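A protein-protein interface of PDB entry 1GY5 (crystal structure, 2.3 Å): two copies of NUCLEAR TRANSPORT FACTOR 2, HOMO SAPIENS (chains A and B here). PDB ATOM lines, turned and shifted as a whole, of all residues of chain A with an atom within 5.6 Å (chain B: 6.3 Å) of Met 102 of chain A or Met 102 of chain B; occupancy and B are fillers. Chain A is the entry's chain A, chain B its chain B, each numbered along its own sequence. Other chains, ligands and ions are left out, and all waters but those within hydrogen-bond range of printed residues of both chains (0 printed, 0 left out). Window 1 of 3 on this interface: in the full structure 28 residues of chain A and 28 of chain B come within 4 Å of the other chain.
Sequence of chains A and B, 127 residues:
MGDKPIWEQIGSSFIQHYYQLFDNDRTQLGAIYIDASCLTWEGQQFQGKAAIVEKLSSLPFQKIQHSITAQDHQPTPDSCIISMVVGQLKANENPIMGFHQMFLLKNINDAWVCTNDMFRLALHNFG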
ATOM      1  N   GLN A  74     -26.545 -27.067  17.066  1.00  0.00           N
ATOM      2  CA  GLN A  74     -26.385 -28.278  16.270  1.00  0.00           C
ATOM      3  C   GLN A  74     -27.242 -29.402  16.824  1.00  0.00           C
ATOM      4  O   GLN A  74     -27.520 -29.469  18.029  1.00  0.00           O
ATOM      5  CB  GLN A  74     -24.932 -28.784  16.262  1.00  0.00           C
ATOM      6  CG  GLN A  74     -23.908 -27.969  15.505  1.00  0.00           C
ATOM      7  CD  GLN A  74     -22.558 -28.654  15.516  1.00  0.00           C
ATOM      8  OE1 GLN A  74     -22.348 -29.592  16.273  1.00  0.00           O
ATOM      9  NE2 GLN A  74     -21.638 -28.191  14.681  1.00  0.00           N
ATOM     10  N   ILE A  81     -29.749 -31.307  21.441  1.00  0.00           N
ATOM     11  CA  ILE A  81     -29.338 -30.076  20.795  1.00  0.00           C
ATOM     12  C   ILE A  81     -28.175 -29.514  21.586  1.00  0.00           C
ATOM     13  O   ILE A  81     -28.228 -29.414  22.806  1.00  0.00           O
ATOM     14  CB  ILE A  81     -30.463 -29.028  20.742  1.00  0.00           C
ATOM     15  CG1 ILE A  81     -31.631 -29.556  19.901  1.00  0.00           C
ATOM     16  CG2 ILE A  81     -29.934 -27.738  20.110  1.00  0.00           C
ATOM     17  CD1 ILE A  81     -32.864 -28.685  19.960  1.00  0.00           C
ATOM     18  N   ILE A  82     -27.110 -29.176  20.878  1.00  0.00           N
ATOM     19  CA  ILE A  82     -25.942 -28.615  21.509  1.00  0.00           C
ATOM     20  C   ILE A  82     -25.832 -27.161  21.070  1.00  0.00           C
ATOM     21  O   ILE A  82     -25.838 -26.858  19.880  1.00  0.00           O
ATOM     22  CB  ILE A  82     -24.684 -29.425  21.129  1.00  0.00           C
ATOM     23  CG1 ILE A  82     -23.451 -28.791  21.763  1.00  0.00           C
ATOM     24  CG2 ILE A  82     -24.572 -29.552  19.625  1.00  0.00           C
ATOM     25  CD1 ILE A  82     -22.665 -29.778  22.591  1.00  0.00           C
ATOM     26  N   SER A  83     -25.787 -26.261  22.050  1.00  0.00           N
ATOM     27  CA  SER A  83     -25.694 -24.831  21.783  1.00  0.00           C
ATOM     28  C   SER A  83     -24.431 -24.240  22.394  1.00  0.00           C
ATOM     29  O   SER A  83     -24.018 -24.629  23.483  1.00  0.00           O
ATOM     30  CB  SER A  83     -26.907 -24.102  22.362  1.00  0.00           C
ATOM     31  OG  SER A  83     -28.127 -24.600  21.840  1.00  0.00           O
ATOM     32  N   MET A  84     -23.811 -23.307  21.685  1.00  0.00           N
ATOM     33  CA  MET A  84     -22.622 -22.648  22.198  1.00  0.00           C
ATOM     34  C   MET A  84     -22.857 -21.154  22.090  1.00  0.00           C
ATOM     35  O   MET A  84     -23.213 -20.650  21.034  1.00  0.00           O
ATOM     36  CB  MET A  84     -21.373 -23.054  21.414  1.00  0.00           C
ATOM     37  CG  MET A  84     -20.104 -22.553  22.071  1.00  0.00           C
ATOM     38  SD  MET A  84     -18.725 -23.713  22.017  1.00  0.00           S
ATOM     39  CE  MET A  84     -17.716 -22.965  20.688  1.00  0.00           C
ATOM     40  N   VAL A  85     -22.672 -20.458  23.205  1.00  0.00           N
ATOM     41  CA  VAL A  85     -22.893 -19.022  23.270  1.00  0.00           C
ATOM     42  C   VAL A  85     -21.634 -18.217  23.618  1.00  0.00           C
ATOM     43  O   VAL A  85     -20.775 -18.674  24.373  1.00  0.00           O
ATOM     44  CB  VAL A  85     -23.978 -18.698  24.337  1.00  0.00           C
ATOM     45  CG1 VAL A  85     -24.187 -17.193  24.436  1.00  0.00           C
ATOM     46  CG2 VAL A  85     -25.287 -19.410  23.992  1.00  0.00           C
ATOM     47  N   HIS A 100     -18.207 -17.502  27.700  1.00  0.00           N
ATOM     48  CA  HIS A 100     -18.713 -18.474  26.752  1.00  0.00           C
ATOM     49  C   HIS A 100     -19.412 -19.569  27.558  1.00  0.00           C
ATOM     50  O   HIS A 100     -18.965 -19.943  28.644  1.00  0.00           O
ATOM     51  CB  HIS A 100     -17.618 -19.048  25.844  1.00  0.00           C
ATOM     52  CG  HIS A 100     -16.526 -19.779  26.558  1.00  0.00           C
ATOM     53  ND1 HIS A 100     -15.443 -19.136  27.119  1.00  0.00           N
ATOM     54  CD2 HIS A 100     -16.301 -21.105  26.714  1.00  0.00           C
ATOM     55  CE1 HIS A 100     -14.594 -20.036  27.583  1.00  0.00           C
ATOM     56  NE2 HIS A 100     -15.091 -21.238  27.350  1.00  0.00           N
ATOM     57  N   GLN A 101     -20.531 -20.055  27.042  1.00  0.00           N
ATOM     58  CA  GLN A 101     -21.284 -21.076  27.741  1.00  0.00           C
ATOM     59  C   GLN A 101     -21.794 -22.137  26.782  1.00  0.00           C
ATOM     60  O   GLN A 101     -22.174 -21.844  25.650  1.00  0.00           O
ATOM     61  CB  GLN A 101     -22.447 -20.419  28.490  1.00  0.00           C
ATOM     62  CG  GLN A 101     -23.250 -21.334  29.386  1.00  0.00           C
ATOM     63  CD  GLN A 101     -23.852 -20.585  30.557  1.00  0.00           C
ATOM     64  OE1 GLN A 101     -24.042 -19.370  30.499  1.00  0.00           O
ATOM     65  NE2 GLN A 101     -24.164 -21.311  31.630  1.00  0.00           N
ATOM     66  N   MET A 102     -21.795 -23.379  27.247  1.00  0.00           N
ATOM     67  CA  MET A 102     -22.248 -24.486  26.432  1.00  0.00           C
ATOM     68  C   MET A 102     -23.414 -25.194  27.102  1.00  0.00           C
ATOM     69  O   MET A 102     -23.373 -25.476  28.296  1.00  0.00           O
ATOM     70  CB  MET A 102     -21.085 -25.447  26.188  1.00  0.00           C
ATOM     71  CG  MET A 102     -21.405 -26.664  25.348  1.00  0.00           C
ATOM     72  SD  MET A 102     -22.162 -27.974  26.314  1.00  0.00           S
ATOM     73  CE  MET A 102     -23.407 -28.469  25.269  1.00  0.00           C
ATOM     74  N   PHE A 103     -24.454 -25.460  26.316  1.00  0.00           N
ATOM     75  CA  PHE A 103     -25.663 -26.136  26.786  1.00  0.00           C
ATOM     76  C   PHE A 103     -25.974 -27.358  25.917  1.00  0.00           C
ATOM     77  O   PHE A 103     -25.991 -27.266  24.676  1.00  0.00           O
ATOM     78  CB  PHE A 103     -26.885 -25.217  26.679  1.00  0.00           C
ATOM     79  CG  PHE A 103     -26.785 -23.928  27.455  1.00  0.00           C
ATOM     80  CD1 PHE A 103     -27.088 -23.890  28.817  1.00  0.00           C
ATOM     81  CD2 PHE A 103     -26.504 -22.735  26.801  1.00  0.00           C
ATOM     82  CE1 PHE A 103     -27.128 -22.668  29.521  1.00  0.00           C
ATOM     83  CE2 PHE A 103     -26.539 -21.517  27.491  1.00  0.00           C
ATOM     84  CZ  PHE A 103     -26.856 -21.487  28.859  1.00  0.00           C
ATOM     85  N   LEU A 104     -26.200 -28.507  26.548  1.00  0.00           N
ATOM     86  CA  LEU A 104     -26.599 -29.680  25.789  1.00  0.00           C
ATOM     87  C   LEU A 104     -28.051 -29.890  26.214  1.00  0.00           C
ATOM     88  O   LEU A 104     -28.346 -29.980  27.402  1.00  0.00           O
ATOM     89  CB  LEU A 104     -25.754 -30.906  26.138  1.00  0.00           C
ATOM     90  CG  LEU A 104     -26.183 -32.128  25.315  1.00  0.00           C
ATOM     91  CD1 LEU A 104     -25.943 -31.852  23.840  1.00  0.00           C
ATOM     92  CD2 LEU A 104     -25.423 -33.376  25.768  1.00  0.00           C
ATOM     93  N   ASN A 116     -26.347 -30.867  30.322  1.00  0.00           N
ATOM     94  CA  ASN A 116     -24.962 -30.428  30.504  1.00  0.00           C
ATOM     95  C   ASN A 116     -24.828 -28.923  30.301  1.00  0.00           C
ATOM     96  O   ASN A 116     -25.352 -28.365  29.330  1.00  0.00           O
ATOM     97  CB  ASN A 116     -24.046 -31.190  29.536  1.00  0.00           C
ATOM     98  CG  ASN A 116     -24.035 -32.686  29.811  1.00  0.00           C
ATOM     99  OD1 ASN A 116     -23.171 -33.188  30.519  1.00  0.00           O
ATOM    100  ND2 ASN A 116     -25.014 -33.391  29.279  1.00  0.00           N
ATOM    101  N   ASP A 117     -24.107 -28.280  31.213  1.00  0.00           N
ATOM    102  CA  ASP A 117     -23.920 -26.827  31.194  1.00  0.00           C
ATOM    103  C   ASP A 117     -22.472 -26.496  31.565  1.00  0.00           C
ATOM    104  O   ASP A 117     -21.970 -26.957  32.593  1.00  0.00           O
ATOM    105  CB  ASP A 117     -24.886 -26.211  32.217  1.00  0.00           C
ATOM    106  CG  ASP A 117     -24.853 -24.681  32.253  1.00  0.00           C
ATOM    107  OD1 ASP A 117     -23.920 -24.041  31.715  1.00  0.00           O
ATOM    108  OD2 ASP A 117     -25.790 -24.116  32.853  1.00  0.00           O
ATOM    109  N   MET A 118     -21.801 -25.716  30.725  1.00  0.00           N
ATOM    110  CA  MET A 118     -20.416 -25.318  30.983  1.00  0.00           C
ATOM    111  C   MET A 118     -20.255 -23.826  30.760  1.00  0.00           C
ATOM    112  O   MET A 118     -20.534 -23.305  29.675  1.00  0.00           O
ATOM    113  CB  MET A 118     -19.447 -26.067  30.065  1.00  0.00           C
ATOM    114  CG  MET A 118     -19.380 -27.559  30.287  1.00  0.00           C
ATOM    115  SD  MET A 118     -18.211 -28.269  29.131  1.00  0.00           S
ATOM    116  CE  MET A 118     -18.241 -30.016  29.610  1.00  0.00           C
ATOM    117  N   PHE A 119     -19.768 -23.148  31.785  1.00  0.00           N
ATOM    118  CA  PHE A 119     -19.595 -21.699  31.752  1.00  0.00           C
ATOM    119  C   PHE A 119     -18.162 -21.297  32.127  1.00  0.00           C
ATOM    120  O   PHE A 119     -17.573 -21.848  33.068  1.00  0.00           O
ATOM    121  CB  PHE A 119     -20.599 -21.060  32.730  1.00  0.00           C
ATOM    122  CG  PHE A 119     -20.489 -19.555  32.841  1.00  0.00           C
ATOM    123  CD1 PHE A 119     -21.155 -18.720  31.951  1.00  0.00           C
ATOM    124  CD2 PHE A 119     -19.691 -18.972  33.823  1.00  0.00           C
ATOM    125  CE1 PHE A 119     -21.028 -17.330  32.039  1.00  0.00           C
ATOM    126  CE2 PHE A 119     -19.562 -17.572  33.912  1.00  0.00           C
ATOM    127  CZ  PHE A 119     -20.230 -16.760  33.021  1.00  0.00           C
ATOM    128  N   GLN B  74     -17.388 -33.601  30.889  1.00  0.00           N
ATOM    129  CA  GLN B  74     -18.584 -34.050  31.593  1.00  0.00           C
ATOM    130  C   GLN B  74     -19.186 -35.236  30.859  1.00  0.00           C
ATOM    131  O   GLN B  74     -18.993 -35.389  29.652  1.00  0.00           O
ATOM    132  CB  GLN B  74     -19.671 -32.960  31.618  1.00  0.00           C
ATOM    133  CG  GLN B  74     -19.365 -31.658  32.334  1.00  0.00           C
ATOM    134  CD  GLN B  74     -20.573 -30.729  32.312  1.00  0.00           C
ATOM    135  OE1 GLN B  74     -21.491 -30.917  31.512  1.00  0.00           O
ATOM    136  NE2 GLN B  74     -20.578 -29.721  33.176  1.00  0.00           N
ATOM    137  N   ILE B  82     -18.817 -34.660  26.771  1.00  0.00           N
ATOM    138  CA  ILE B  82     -18.700 -33.304  26.254  1.00  0.00           C
ATOM    139  C   ILE B  82     -17.423 -32.679  26.779  1.00  0.00           C
ATOM    140  O   ILE B  82     -17.145 -32.745  27.984  1.00  0.00           O
ATOM    141  CB  ILE B  82     -19.833 -32.397  26.730  1.00  0.00           C
ATOM    142  CG1 ILE B  82     -21.178 -32.962  26.306  1.00  0.00           C
ATOM    143  CG2 ILE B  82     -19.640 -31.002  26.149  1.00  0.00           C
ATOM    144  CD1 ILE B  82     -22.335 -32.193  26.870  1.00  0.00           C
ATOM    145  N   SER B  83     -16.659 -32.069  25.878  1.00  0.00           N
ATOM    146  CA  SER B  83     -15.420 -31.404  26.242  1.00  0.00           C
ATOM    147  C   SER B  83     -15.457 -29.965  25.750  1.00  0.00           C
ATOM    148  O   SER B  83     -15.804 -29.703  24.598  1.00  0.00           O
ATOM    149  CB  SER B  83     -14.219 -32.103  25.615  1.00  0.00           C
ATOM    150  OG  SER B  83     -14.140 -33.456  26.014  1.00  0.00           O
ATOM    151  N   MET B  84     -15.111 -29.038  26.637  1.00  0.00           N
ATOM    152  CA  MET B  84     -15.067 -27.627  26.303  1.00  0.00           C
ATOM    153  C   MET B  84     -13.609 -27.219  26.458  1.00  0.00           C
ATOM    154  O   MET B  84     -13.032 -27.328  27.541  1.00  0.00           O
ATOM    155  CB  MET B  84     -15.935 -26.825  27.261  1.00  0.00           C
ATOM    156  CG  MET B  84     -16.082 -25.373  26.865  1.00  0.00           C
ATOM    157  SD  MET B  84     -17.349 -25.097  25.609  1.00  0.00           S
ATOM    158  CE  MET B  84     -18.355 -23.920  26.475  1.00  0.00           C
ATOM    159  N   VAL B  85     -13.008 -26.762  25.367  1.00  0.00           N
ATOM    160  CA  VAL B  85     -11.610 -26.356  25.377  1.00  0.00           C
ATOM    161  C   VAL B  85     -11.450 -24.863  25.082  1.00  0.00           C
ATOM    162  O   VAL B  85     -12.217 -24.280  24.303  1.00  0.00           O
ATOM    163  CB  VAL B  85     -10.799 -27.169  24.320  1.00  0.00           C
ATOM    164  CG1 VAL B  85      -9.395 -26.643  24.207  1.00  0.00           C
ATOM    165  CG2 VAL B  85     -10.761 -28.633  24.700  1.00  0.00           C
ATOM    166  N   HIS B 100     -11.906 -21.115  21.131  1.00  0.00           N
ATOM    167  CA  HIS B 100     -12.814 -21.907  21.964  1.00  0.00           C
ATOM    168  C   HIS B 100     -13.260 -23.090  21.103  1.00  0.00           C
ATOM    169  O   HIS B 100     -13.486 -22.929  19.912  1.00  0.00           O
ATOM    170  CB  HIS B 100     -14.078 -21.108  22.334  1.00  0.00           C
ATOM    171  CG  HIS B 100     -13.835 -19.921  23.214  1.00  0.00           C
ATOM    172  ND1 HIS B 100     -14.854 -19.086  23.620  1.00  0.00           N
ATOM    173  CD2 HIS B 100     -12.711 -19.454  23.802  1.00  0.00           C
ATOM    174  CE1 HIS B 100     -14.368 -18.158  24.426  1.00  0.00           C
ATOM    175  NE2 HIS B 100     -13.070 -18.358  24.555  1.00  0.00           N
ATOM    176  N   GLN B 101     -13.402 -24.272  21.683  1.00  0.00           N
ATOM    177  CA  GLN B 101     -13.860 -25.404  20.890  1.00  0.00           C
ATOM    178  C   GLN B 101     -14.630 -26.422  21.725  1.00  0.00           C
ATOM    179  O   GLN B 101     -14.280 -26.711  22.866  1.00  0.00           O
ATOM    180  CB  GLN B 101     -12.678 -26.057  20.168  1.00  0.00           C
ATOM    181  CG  GLN B 101     -13.078 -27.135  19.176  1.00  0.00           C
ATOM    182  CD  GLN B 101     -11.983 -27.424  18.152  1.00  0.00           C
ATOM    183  OE1 GLN B 101     -10.793 -27.250  18.429  1.00  0.00           O
ATOM    184  NE2 GLN B 101     -12.385 -27.888  16.970  1.00  0.00           N
ATOM    185  N   MET B 102     -15.696 -26.953  21.141  1.00  0.00           N
ATOM    186  CA  MET B 102     -16.551 -27.926  21.812  1.00  0.00           C
ATOM    187  C   MET B 102     -16.545 -29.240  21.033  1.00  0.00           C
ATOM    188  O   MET B 102     -16.607 -29.241  19.812  1.00  0.00           O
ATOM    189  CB  MET B 102     -17.976 -27.345  21.912  1.00  0.00           C
ATOM    190  CG  MET B 102     -19.042 -28.214  22.599  1.00  0.00           C
ATOM    191  SD  MET B 102     -19.520 -29.698  21.670  1.00  0.00           S
ATOM    192  CE  MET B 102     -20.366 -28.957  20.248  1.00  0.00           C
ATOM    193  N   PHE B 103     -16.445 -30.352  21.747  1.00  0.00           N
ATOM    194  CA  PHE B 103     -16.447 -31.681  21.141  1.00  0.00           C
ATOM    195  C   PHE B 103     -17.448 -32.562  21.878  1.00  0.00           C
ATOM    196  O   PHE B 103     -17.447 -32.604  23.101  1.00  0.00           O
ATOM    197  CB  PHE B 103     -15.081 -32.369  21.279  1.00  0.00           C
ATOM    198  CG  PHE B 103     -13.959 -31.682  20.569  1.00  0.00           C
ATOM    199  CD1 PHE B 103     -13.804 -31.814  19.192  1.00  0.00           C
ATOM    200  CD2 PHE B 103     -13.024 -30.933  21.288  1.00  0.00           C
ATOM    201  CE1 PHE B 103     -12.719 -31.211  18.533  1.00  0.00           C
ATOM    202  CE2 PHE B 103     -11.946 -30.329  20.645  1.00  0.00           C
ATOM    203  CZ  PHE B 103     -11.789 -30.470  19.258  1.00  0.00           C
ATOM    204  N   LEU B 104     -18.316 -33.244  21.143  1.00  0.00           N
ATOM    205  CA  LEU B 104     -19.231 -34.185  21.769  1.00  0.00           C
ATOM    206  C   LEU B 104     -18.674 -35.506  21.250  1.00  0.00           C
ATOM    207  O   LEU B 104     -18.478 -35.676  20.047  1.00  0.00           O
ATOM    208  CB  LEU B 104     -20.674 -33.981  21.308  1.00  0.00           C
ATOM    209  CG  LEU B 104     -21.679 -34.988  21.888  1.00  0.00           C
ATOM    210  CD1 LEU B 104     -21.667 -34.916  23.399  1.00  0.00           C
ATOM    211  CD2 LEU B 104     -23.074 -34.705  21.352  1.00  0.00           C
ATOM    212  N   CYS B 114     -15.927 -38.174  17.393  1.00  0.00           N
ATOM    213  CA  CYS B 114     -16.571 -36.878  17.520  1.00  0.00           C
ATOM    214  C   CYS B 114     -17.786 -36.737  16.611  1.00  0.00           C
ATOM    215  O   CYS B 114     -17.654 -36.784  15.392  1.00  0.00           O
ATOM    216  CB  CYS B 114     -15.576 -35.768  17.182  1.00  0.00           C
ATOM    217  SG  CYS B 114     -16.280 -34.127  17.403  1.00  0.00           S
ATOM    218  N   ASN B 116     -20.033 -34.083  17.164  1.00  0.00           N
ATOM    219  CA  ASN B 116     -20.297 -32.644  17.114  1.00  0.00           C
ATOM    220  C   ASN B 116     -19.055 -31.844  17.475  1.00  0.00           C
ATOM    221  O   ASN B 116     -18.374 -32.121  18.473  1.00  0.00           O
ATOM    222  CB  ASN B 116     -21.451 -32.292  18.058  1.00  0.00           C
ATOM    223  CG  ASN B 116     -22.783 -32.814  17.563  1.00  0.00           C
ATOM    224  OD1 ASN B 116     -23.545 -32.091  16.921  1.00  0.00           O
ATOM    225  ND2 ASN B 116     -23.065 -34.076  17.844  1.00  0.00           N
ATOM    226  N   ASP B 117     -18.784 -30.825  16.670  1.00  0.00           N
ATOM    227  CA  ASP B 117     -17.596 -30.014  16.845  1.00  0.00           C
ATOM    228  C   ASP B 117     -17.919 -28.564  16.528  1.00  0.00           C
ATOM    229  O   ASP B 117     -18.416 -28.244  15.447  1.00  0.00           O
ATOM    230  CB  ASP B 117     -16.513 -30.577  15.908  1.00  0.00           C
ATOM    231  CG  ASP B 117     -15.220 -29.767  15.903  1.00  0.00           C
ATOM    232  OD1 ASP B 117     -15.099 -28.764  16.628  1.00  0.00           O
ATOM    233  OD2 ASP B 117     -14.305 -30.154  15.151  1.00  0.00           O
ATOM    234  N   MET B 118     -17.669 -27.689  17.491  1.00  0.00           N
ATOM    235  CA  MET B 118     -17.911 -26.269  17.296  1.00  0.00           C
ATOM    236  C   MET B 118     -16.639 -25.522  17.643  1.00  0.00           C
ATOM    237  O   MET B 118     -16.075 -25.701  18.715  1.00  0.00           O
ATOM    238  CB  MET B 118     -19.096 -25.790  18.147  1.00  0.00           C
ATOM    239  CG  MET B 118     -20.450 -26.256  17.598  1.00  0.00           C
ATOM    240  SD  MET B 118     -21.900 -25.662  18.511  1.00  0.00           S
ATOM    241  CE  MET B 118     -22.860 -27.105  18.538  1.00  0.00           C
ATOM    242  N   PHE B 119     -16.195 -24.687  16.710  1.00  0.00           N
ATOM    243  CA  PHE B 119     -14.961 -23.921  16.846  1.00  0.00           C
ATOM    244  C   PHE B 119     -15.207 -22.445  16.581  1.00  0.00           C
ATOM    245  O   PHE B 119     -15.976 -22.072  15.686  1.00  0.00           O
ATOM    246  CB  PHE B 119     -13.930 -24.453  15.851  1.00  0.00           C
ATOM    247  CG  PHE B 119     -12.647 -23.681  15.824  1.00  0.00           C
ATOM    248  CD1 PHE B 119     -11.615 -23.983  16.710  1.00  0.00           C
ATOM    249  CD2 PHE B 119     -12.458 -22.662  14.897  1.00  0.00           C
ATOM    250  CE1 PHE B 119     -10.414 -23.286  16.672  1.00  0.00           C
ATOM    251  CE2 PHE B 119     -11.256 -21.960  14.854  1.00  0.00           C
ATOM    252  CZ  PHE B 119     -10.234 -22.275  15.744  1.00  0.00           C
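O of Asp 117 of chain B lies within hydrogen-bond range of NE2 of Gln 74 of chain A, 3.3 Å away.
The backbone carbonyl oxygen (O) of Asp 117 of chain A is in hydrogen-bond range of the side-chain amide nitrogen (NE2) of Gln 74 of chain B, at 3.1 Å.
The side-chain amide oxygen (OE1) of Gln 74 of chain A sits close to the side-chain amide oxygen (OD1) of Asn 116 of chain B, at 2.8 Å.
OD1 of Asn 116 of chain A lies close to OE1 of Gln 74 of chain B.
N of Ile 82 of chain B lies within hydrogen-bond range of O of Gln 74 of chain B (3.0 Å).
The side-chain amide nitrogen (NE2) of Gln 101 of chain B lies within hydrogen-bond range of the side-chain carboxylate (OD1) of Asp 117 of chain B (2.9 Å).
The backbone carbonyl oxygen of Gln 74 of chain A sits at hydrogen-bond distance from the backbone NH of Ile 82 of chain A, 2.9 Å away.
N of Leu 104 of chain B lies within hydrogen-bond range of O of Asn 116 of chain B (2.9 Å).
The backbone NH (N) of Met 102 of chain B sits at hydrogen-bond distance from the backbone carbonyl oxygen (O) of Met 118 of chain B, at 2.8 Å.
The backbone NH (N) of Met 102 of chain A is in hydrogen-bond range of the backbone carbonyl oxygen (O) of Met 118 of chain A (2.7 Å).
Met 118 of chain B touches Gln 74 of chain A.
Ile 82 of chain A touches Met 102 of chain B (CD1 to SD, 3.3 Å).
CG2 of Ile 82 of chain A touches OD1 of Asn 116 of chain B, at 3.8 Å.
CG2 of Ile 82 of chain A touches CE of Met 118 of chain B, 3.2 Å away.
CE1 of His 100 of chain B touches ND1 of His 100 of chain A, 3.1 Å away.
SD of Met 102 of chain A touches CG2 of Ile 82 of chain B, at 3.9 Å.
Met 84 of chain B touches Met 102 of chain A.
Ile 82 of chain B touches Leu 104 of chain A (CD1 to CD2, 3.5 Å).
Asn 116 of chain A touches Ile 82 of chain B (CB to CD1, 3.3 Å).
Met 118 of chain A touches Ile 82 of chain B (CE to O, 3.4 Å).
Of the printed residues of chain B, Ile 82 of chain A touches Met 102, Asn 116 and Met 118.
Of the printed residues of chain B, Met 84 of chain A touches Met 102 (3.7 Å) and Met 118 (3.8 Å).
Printed residues of chain B within 4 Å of His 100 of chain A: Met 84 (3.5 Å) and His 100 (3.1 Å).
Of the printed residues of chain B, Gln 101 of chain A touches Met 84.
Met 102 of chain A touches just these residues of chain B: Ile 82 (3.9 Å), Met 84 (3.1 Å) and Met 102 (3.9 Å).
Of the printed residues of chain B, Asn 116 of chain A touches Gln 74 and Ile 82.
Of chain A, only Ile 82 (3.3 Å), Met 84 (3.7 Å) and Met 102 (3.9 Å) come within 4 Å of Met 102 of chain B.
Leu 104 of chain B touches none of the printed residues of chain A.
The nearest residue of chain A that does not touch Met 102 of chain B is Gln 74 of chain A (4.5 Å).
Hydrophobic or aromatic side chains of chain A within 4 Å of the printed part of chain B: Ile 82, Met 84, His 100, Met 102, Leu 104 and Met 118.
Of the 15 printed residues of chain B, 8 touch a printed residue of chain A.
Printed residues of chain B that touch a printed residue of chain A: Gln 74, Ile 82, Met 84, His 100, Met 102, Asn 116, Asp 117 and Met 118.
Hydrophobic or aromatic side chains of chain B that line the printed part of chain A: Ile 82, Met 84, His 100, Met 102 and Met 118.
Among the printed residues, 21 pairs touch across the chains.
Among the printed residues, no Asp or Glu carboxylate lies within 4 Å of a Lys or Arg side-chain nitrogen of the other chain.
Ile 82 of chain A touches Asn 116 of chain B, and with the chains exchanged Asn 116 of chain A touches Ile 82 of chain B.
Ile 82 of chain A touches Met 118 of chain B, and with the chains exchanged Met 118 of chain A touches Ile 82 of chain B.
His 100 of chain A touches Met 84 of chain B, but with the chains exchanged Met 84 of chain A does not touch His 100 of chain B (4.3 Å).
Gln 101 of chain A touches Met 84 of chain B, but with the chains exchanged Met 84 of chain A does not touch Gln 101 of chain B (4.6 Å).
Positions printed for both chains: 74, 82, 83, 84, 85, 100, 101, 102, 103, 104, 116, 117, 118 and 119.
Of the 21 pairs that touch across the chains among the printed residues, 18 have their exchanged pair printed and touching as well.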
